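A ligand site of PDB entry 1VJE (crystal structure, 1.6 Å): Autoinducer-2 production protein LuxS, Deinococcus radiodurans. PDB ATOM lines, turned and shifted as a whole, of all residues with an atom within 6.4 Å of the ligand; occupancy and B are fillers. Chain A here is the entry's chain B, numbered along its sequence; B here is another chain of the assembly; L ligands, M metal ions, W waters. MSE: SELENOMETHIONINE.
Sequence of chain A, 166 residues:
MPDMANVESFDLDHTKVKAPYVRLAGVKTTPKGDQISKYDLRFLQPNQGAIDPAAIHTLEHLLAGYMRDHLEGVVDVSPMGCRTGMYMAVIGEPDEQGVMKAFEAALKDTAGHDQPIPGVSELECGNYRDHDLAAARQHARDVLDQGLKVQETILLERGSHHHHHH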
ATOM      1  N   HIS A  57      -9.074 -12.531  17.167  1.00  0.00           N
ATOM      2  CA  HIS A  57      -9.491 -11.617  16.081  1.00  0.00           C
ATOM      3  C   HIS A  57      -8.224 -11.176  15.343  1.00  0.00           C
ATOM      4  O   HIS A  57      -8.156 -11.179  14.123  1.00  0.00           O
ATOM      5  CB  HIS A  57     -10.201 -10.437  16.699  1.00  0.00           C
ATOM      6  CG  HIS A  57     -10.799  -9.509  15.707  1.00  0.00           C
ATOM      7  ND1 HIS A  57     -11.172  -8.237  16.130  1.00  0.00           N
ATOM      8  CD2 HIS A  57     -11.106  -9.596  14.388  1.00  0.00           C
ATOM      9  CE1 HIS A  57     -11.720  -7.586  15.106  1.00  0.00           C
ATOM     10  NE2 HIS A  57     -11.679  -8.382  14.069  1.00  0.00           N
ATOM     11  N   GLU A  60      -6.936 -14.036  13.302  1.00  0.00           N
ATOM     12  CA  GLU A  60      -7.715 -14.190  12.065  1.00  0.00           C
ATOM     13  C   GLU A  60      -7.227 -13.216  11.004  1.00  0.00           C
ATOM     14  O   GLU A  60      -6.963 -13.590   9.865  1.00  0.00           O
ATOM     15  CB  GLU A  60      -9.177 -13.855  12.433  1.00  0.00           C
ATOM     16  CG  GLU A  60     -10.115 -13.780  11.223  1.00  0.00           C
ATOM     17  CD  GLU A  60     -11.405 -13.069  11.606  1.00  0.00           C
ATOM     18  OE1 GLU A  60     -11.323 -11.913  12.113  1.00  0.00           O
ATOM     19  OE2 GLU A  60     -12.485 -13.649  11.371  1.00  0.00           O
ATOM     20  N   HIS A  61      -7.030 -11.933  11.344  1.00  0.00           N
ATOM     21  CA  HIS A  61      -6.540 -10.986  10.331  1.00  0.00           C
ATOM     22  C   HIS A  61      -5.136 -11.376   9.851  1.00  0.00           C
ATOM     23  O   HIS A  61      -4.867 -11.286   8.650  1.00  0.00           O
ATOM     24  CB  HIS A  61      -6.427  -9.586  10.961  1.00  0.00           C
ATOM     25  CG  HIS A  61      -7.750  -8.864  11.022  1.00  0.00           C
ATOM     26  ND1 HIS A  61      -7.857  -7.566  10.532  1.00  0.00           N
ATOM     27  CD2 HIS A  61      -8.943  -9.209  11.500  1.00  0.00           C
ATOM     28  CE1 HIS A  61      -9.107  -7.143  10.725  1.00  0.00           C
ATOM     29  NE2 HIS A  61      -9.788  -8.103  11.313  1.00  0.00           N
ATOM     30  N   LEU A  62      -4.269 -11.818  10.758  1.00  0.00           N
ATOM     31  CA  LEU A  62      -2.915 -12.156  10.308  1.00  0.00           C
ATOM     32  C   LEU A  62      -2.855 -13.434   9.521  1.00  0.00           C
ATOM     33  O   LEU A  62      -2.188 -13.495   8.490  1.00  0.00           O
ATOM     34  CB  LEU A  62      -1.975 -12.312  11.538  1.00  0.00           C
ATOM     35  CG  LEU A  62      -1.715 -10.991  12.264  1.00  0.00           C
ATOM     36  CD1 LEU A  62      -0.973 -11.227  13.560  1.00  0.00           C
ATOM     37  CD2 LEU A  62      -0.981 -10.001  11.382  1.00  0.00           C
ATOM     38  N   ALA A  64      -5.223 -14.907   7.888  1.00  0.00           N
ATOM     39  CA  ALA A  64      -5.973 -14.799   6.624  1.00  0.00           C
ATOM     40  C   ALA A  64      -4.965 -14.549   5.504  1.00  0.00           C
ATOM     41  O   ALA A  64      -5.031 -15.103   4.403  1.00  0.00           O
ATOM     42  CB  ALA A  64      -6.963 -13.664   6.703  1.00  0.00           C
ATOM     43  N   ARG A  68      -2.552 -17.562   3.062  1.00  0.00           N
ATOM     44  CA  ARG A  68      -2.644 -17.348   1.600  1.00  0.00           C
ATOM     45  C   ARG A  68      -1.269 -17.156   0.988  1.00  0.00           C
ATOM     46  O   ARG A  68      -0.971 -17.620  -0.138  1.00  0.00           O
ATOM     47  CB  ARG A  68      -3.577 -16.185   1.293  1.00  0.00           C
ATOM     48  CG  ARG A  68      -5.060 -16.460   1.525  1.00  0.00           C
ATOM     49  CD  ARG A  68      -5.902 -15.262   1.178  1.00  0.00           C
ATOM     50  NE  ARG A  68      -7.323 -15.521   1.187  1.00  0.00           N
ATOM     51  CZ  ARG A  68      -8.191 -15.626   2.148  1.00  0.00           C
ATOM     52  NH1 ARG A  68      -9.482 -15.870   1.865  1.00  0.00           N
ATOM     53  NH2 ARG A  68      -7.854 -15.501   3.437  1.00  0.00           N
ATOM     54  N   VAL A  74      -6.428 -21.180  -0.912  1.00  0.00           N
ATOM     55  CA  VAL A  74      -7.142 -20.904   0.369  1.00  0.00           C
ATOM     56  C   VAL A  74      -8.451 -20.193   0.113  1.00  0.00           C
ATOM     57  O   VAL A  74      -8.428 -19.122  -0.523  1.00  0.00           O
ATOM     58  CB  VAL A  74      -6.231 -20.051   1.273  1.00  0.00           C
ATOM     59  CG1 VAL A  74      -6.979 -19.733   2.575  1.00  0.00           C
ATOM     60  CG2 VAL A  74      -4.967 -20.836   1.592  1.00  0.00           C
ATOM     61  N   VAL A  75      -9.537 -20.650   0.725  1.00  0.00           N
ATOM     62  CA  VAL A  75     -10.840 -20.010   0.532  1.00  0.00           C
ATOM     63  C   VAL A  75     -11.138 -19.113   1.723  1.00  0.00           C
ATOM     64  O   VAL A  75     -11.743 -18.066   1.548  1.00  0.00           O
ATOM     65  CB  VAL A  75     -11.937 -21.087   0.372  1.00  0.00           C
ATOM     66  CG1 VAL A  75     -13.339 -20.622   0.709  1.00  0.00           C
ATOM     67  CG2 VAL A  75     -11.941 -21.573  -1.087  1.00  0.00           C
ATOM     68  N   ASP A  76     -10.743 -19.601   2.909  1.00  0.00           N
ATOM     69  CA  ASP A  76     -11.051 -18.852   4.117  1.00  0.00           C
ATOM     70  C   ASP A  76     -10.246 -19.319   5.317  1.00  0.00           C
ATOM     71  O   ASP A  76      -9.860 -20.493   5.373  1.00  0.00           O
ATOM     72  CB  ASP A  76     -12.531 -19.271   4.410  1.00  0.00           C
ATOM     73  CG  ASP A  76     -13.091 -18.547   5.622  1.00  0.00           C
ATOM     74  OD1 ASP A  76     -13.381 -17.352   5.473  1.00  0.00           O
ATOM     75  OD2 ASP A  76     -13.207 -19.209   6.692  1.00  0.00           O
ATOM     76  N   VAL A  77      -9.998 -18.423   6.255  1.00  0.00           N
ATOM     77  CA  VAL A  77      -9.363 -18.758   7.548  1.00  0.00           C
ATOM     78  C   VAL A  77     -10.263 -18.107   8.617  1.00  0.00           C
ATOM     79  O   VAL A  77     -10.426 -16.873   8.640  1.00  0.00           O
ATOM     80  CB  VAL A  77      -7.948 -18.229   7.752  1.00  0.00           C
ATOM     81  CG1 VAL A  77      -7.482 -18.615   9.162  1.00  0.00           C
ATOM     82  CG2 VAL A  77      -6.955 -18.828   6.759  1.00  0.00           C
ATOM     83  N   SER A  78     -10.959 -18.915   9.420  1.00  0.00           N
ATOM     84  CA  SER A  78     -11.868 -18.352  10.423  1.00  0.00           C
ATOM     85  C   SER A  78     -11.550 -18.859  11.829  1.00  0.00           C
ATOM     86  O   SER A  78     -11.049 -19.962  12.018  1.00  0.00           O
ATOM     87  CB  SER A  78     -13.294 -18.906  10.110  1.00  0.00           C
ATOM     88  OG  SER A  78     -13.795 -18.074   9.038  1.00  0.00           O
ATOM     89  N   PRO A  79     -11.814 -18.034  12.830  1.00  0.00           N
ATOM     90  CA  PRO A  79     -11.613 -18.500  14.202  1.00  0.00           C
ATOM     91  C   PRO A  79     -12.705 -19.487  14.570  1.00  0.00           C
ATOM     92  O   PRO A  79     -13.865 -19.380  14.085  1.00  0.00           O
ATOM     93  CB  PRO A  79     -11.800 -17.211  14.999  1.00  0.00           C
ATOM     94  CG  PRO A  79     -12.774 -16.394  14.191  1.00  0.00           C
ATOM     95  CD  PRO A  79     -12.399 -16.693  12.765  1.00  0.00           C
ATOM     96  N   GLU A 124     -12.466  -0.960   7.565  1.00  0.00           N
ATOM     97  CA  GLU A 124     -12.119  -2.281   7.160  1.00  0.00           C
ATOM     98  C   GLU A 124     -12.439  -3.447   8.078  1.00  0.00           C
ATOM     99  O   GLU A 124     -12.332  -4.579   7.599  1.00  0.00           O
ATOM    100  CB  GLU A 124     -10.566  -2.314   7.007  1.00  0.00           C
ATOM    101  CG  GLU A 124     -10.006  -1.417   5.906  1.00  0.00           C
ATOM    102  CD  GLU A 124      -8.481  -1.285   6.091  1.00  0.00           C
ATOM    103  OE1 GLU A 124      -8.099  -0.709   7.127  1.00  0.00           O
ATOM    104  OE2 GLU A 124      -7.763  -1.811   5.214  1.00  0.00           O
ATOM    105  N   GLU B   8     -11.905  -8.917  -1.108  1.00  0.00           N
ATOM    106  CA  GLU B   8     -11.472  -9.357   0.216  1.00  0.00           C
ATOM    107  C   GLU B   8     -12.186  -8.567   1.308  1.00  0.00           C
ATOM    108  O   GLU B   8     -12.629  -7.458   1.222  1.00  0.00           O
ATOM    109  CB  GLU B   8      -9.958  -9.194   0.362  1.00  0.00           C
ATOM    110  CG  GLU B   8      -9.287 -10.334   1.120  1.00  0.00           C
ATOM    111  CD  GLU B   8      -7.985 -10.761   0.484  1.00  0.00           C
ATOM    112  OE1 GLU B   8      -7.996 -11.742  -0.292  1.00  0.00           O
ATOM    113  OE2 GLU B   8      -6.943 -10.127   0.762  1.00  0.00           O
ATOM    114  N   SER B   9     -12.197  -9.260   2.495  1.00  0.00           N
ATOM    115  CA  SER B   9     -12.805  -8.759   3.685  1.00  0.00           C
ATOM    116  C   SER B   9     -12.418  -7.332   4.019  1.00  0.00           C
ATOM    117  O   SER B   9     -13.295  -6.499   4.318  1.00  0.00           O
ATOM    118  CB  SER B   9     -12.461  -9.658   4.903  1.00  0.00           C
ATOM    119  OG  SER B   9     -13.056  -9.092   6.054  1.00  0.00           O
ATOM    120  N   PHE B  10     -11.142  -6.957   3.909  1.00  0.00           N
ATOM    121  CA  PHE B  10     -10.734  -5.588   4.217  1.00  0.00           C
ATOM    122  C   PHE B  10     -11.146  -4.562   3.170  1.00  0.00           C
ATOM    123  O   PHE B  10     -10.910  -3.370   3.422  1.00  0.00           O
ATOM    124  CB  PHE B  10      -9.219  -5.504   4.424  1.00  0.00           C
ATOM    125  CG  PHE B  10      -8.651  -6.493   5.391  1.00  0.00           C
ATOM    126  CD1 PHE B  10      -7.339  -6.915   5.219  1.00  0.00           C
ATOM    127  CD2 PHE B  10      -9.359  -6.981   6.476  1.00  0.00           C
ATOM    128  CE1 PHE B  10      -6.732  -7.807   6.105  1.00  0.00           C
ATOM    129  CE2 PHE B  10      -8.764  -7.874   7.349  1.00  0.00           C
ATOM    130  CZ  PHE B  10      -7.462  -8.311   7.163  1.00  0.00           C
ATOM    131  N   LYS B  38     -19.092 -17.461  -0.821  1.00  0.00           N
ATOM    132  CA  LYS B  38     -18.903 -17.133   0.606  1.00  0.00           C
ATOM    133  C   LYS B  38     -19.960 -16.096   0.987  1.00  0.00           C
ATOM    134  O   LYS B  38     -20.111 -15.143   0.221  1.00  0.00           O
ATOM    135  CB  LYS B  38     -17.520 -16.522   0.869  1.00  0.00           C
ATOM    136  CG  LYS B  38     -17.313 -16.383   2.394  1.00  0.00           C
ATOM    137  CD  LYS B  38     -15.946 -15.710   2.653  1.00  0.00           C
ATOM    138  CE  LYS B  38     -14.839 -16.736   2.375  1.00  0.00           C
ATOM    139  NZ  LYS B  38     -13.536 -16.229   2.905  1.00  0.00           N
ATOM    140  N   GLY B  81     -14.224 -13.124  13.495  1.00  0.00           N
ATOM    141  CA  GLY B  81     -13.430 -12.615  14.634  1.00  0.00           C
ATOM    142  C   GLY B  81     -13.977 -11.318  15.185  1.00  0.00           C
ATOM    143  O   GLY B  81     -13.841 -11.016  16.383  1.00  0.00           O
ATOM    144  N   CSD B  82     -14.611 -10.459  14.351  1.00  0.00           N
ATOM    145  CA  CSD B  82     -15.177  -9.214  14.818  1.00  0.00           C
ATOM    146  CB  CSD B  82     -15.387  -8.260  13.652  1.00  0.00           C
ATOM    147  SG  CSD B  82     -16.370  -8.933  12.270  1.00  0.00           S
ATOM    148  C   CSD B  82     -16.484  -9.397  15.588  1.00  0.00           C
ATOM    149  O   CSD B  82     -17.021  -8.449  16.108  1.00  0.00           O
ATOM    150  OD1 CSD B  82     -17.734  -9.229  12.869  1.00  0.00           O
ATOM    151  OD2 CSD B  82     -16.505  -7.821  11.295  1.00  0.00           O
ATOM    152  N   TYR B  87     -19.555 -16.142   8.954  1.00  0.00           N
ATOM    153  CA  TYR B  87     -19.240 -16.403   7.544  1.00  0.00           C
ATOM    154  C   TYR B  87     -19.746 -17.807   7.203  1.00  0.00           C
ATOM    155  O   TYR B  87     -19.693 -18.736   8.037  1.00  0.00           O
ATOM    156  CB  TYR B  87     -17.753 -16.336   7.240  1.00  0.00           C
ATOM    157  CG  TYR B  87     -17.270 -15.015   6.661  1.00  0.00           C
ATOM    158  CD1 TYR B  87     -17.797 -14.466   5.502  1.00  0.00           C
ATOM    159  CD2 TYR B  87     -16.264 -14.309   7.313  1.00  0.00           C
ATOM    160  CE1 TYR B  87     -17.333 -13.248   5.027  1.00  0.00           C
ATOM    161  CE2 TYR B  87     -15.775 -13.108   6.841  1.00  0.00           C
ATOM    162  CZ  TYR B  87     -16.334 -12.587   5.682  1.00  0.00           C
ATOM    163  OH  TYR B  87     -15.868 -11.383   5.206  1.00  0.00           O
HETATM  164  N   MSE L   1     -12.539 -15.576   7.161  1.00  0.00           N
HETATM  165  CA  MSE L   1     -11.956 -14.553   6.319  1.00  0.00           C
HETATM  166  C   MSE L   1     -11.249 -15.142   5.102  1.00  0.00           C
HETATM  167  O   MSE L   1     -10.164 -15.727   5.287  1.00  0.00           O
HETATM  168  OXT MSE L   1     -11.447 -14.526   4.000  1.00  0.00           O
HETATM  169  CB  MSE L   1     -10.939 -13.794   7.207  1.00  0.00           C
HETATM  170  CG  MSE L   1     -10.432 -12.532   6.552  1.00  0.00           C
HETATM  171 SE   MSE L   1      -9.807 -11.348   7.896  1.00  0.00          SE
HETATM  172  CE  MSE L   1     -11.415 -10.682   8.669  1.00  0.00           C
HETATM  173 ZN    ZN M   1     -11.625  -7.470  12.194  1.00  0.00          ZN
HETATM  174  O   HOH W   1     -14.524 -11.637   9.468  1.00  0.00           O
HETATM  175  O   HOH W   2     -13.809 -14.611   9.403  1.00  0.00           O
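OD1 of Asp 76 lies within salt-bridge range of N of the ligand (2.6 Å).
An oxygen (O) of the ligand is in hydrogen-bond range of the backbone NH (N) of Val 77 (2.9 Å).
A nitrogen (N) of the ligand sits at hydrogen-bond distance from the backbone carbonyl oxygen of Val 77 (2.9 Å).
NZ of Lys 38 of chain B is in salt-bridge range of OXT of the ligand (2.9 Å).
The guanidinium group (NH2) of Arg 68 is in salt-bridge range of an oxygen (O) of the ligand, 3.0 Å away.
The side-chain hydroxyl (OG) of Ser 78 lies within hydrogen-bond range of a nitrogen (N) of the ligand, 3.4 Å away.
OD1 of Asp 76 lies within salt-bridge range of NZ of Lys 38 of chain B.
OD2 of Asp 76 sits at hydrogen-bond distance from OG of Ser 78 (2.7 Å).
The side-chain amino group (NZ) of Lys 38 of chain B is in hydrogen-bond range of the backbone carbonyl oxygen (O) of Val 75 (2.9 Å).
O of Ala 64 is in hydrogen-bond range of NH2 of Arg 68 (3.0 Å).
The guanidinium group of Arg 68 sits at hydrogen-bond distance from the backbone carbonyl oxygen of Val 75 (3.2 Å).
OE2 of Glu 60 sits at hydrogen-bond distance from N of Gly 81 of chain B, 2.8 Å away.
Glu 60 touches the ligand.
Ala 64 touches the ligand (CB to CG, 3.7 Å).
Ser 9 of chain B touches the ligand.
CE2 of Phe 10 of chain B touches SE of the ligand, 3.7 Å away.
CD2 of Tyr 87 of chain B touches N of the ligand, at 3.9 Å.
Hydrophobic or aromatic side chains that line the ligand: Ala 64, Phe 10 of chain B and Tyr 87 of chain B.
Ten residues have an atom within 4 Å of the ligand: Glu 60, Ala 64, Arg 68, Asp 76, Val 77, Ser 78, Ser 9 of chain B, Phe 10 of chain B, Lys 38 of chain B and Tyr 87 of chain B.
Water W2 lies within hydrogen-bond range of the side-chain carboxylate (OE2) of Glu 60 (2.6 Å), a nitrogen (N) of the ligand (2.8 Å) and the side-chain hydroxyl (OG) of Ser 78 (3.5 Å).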
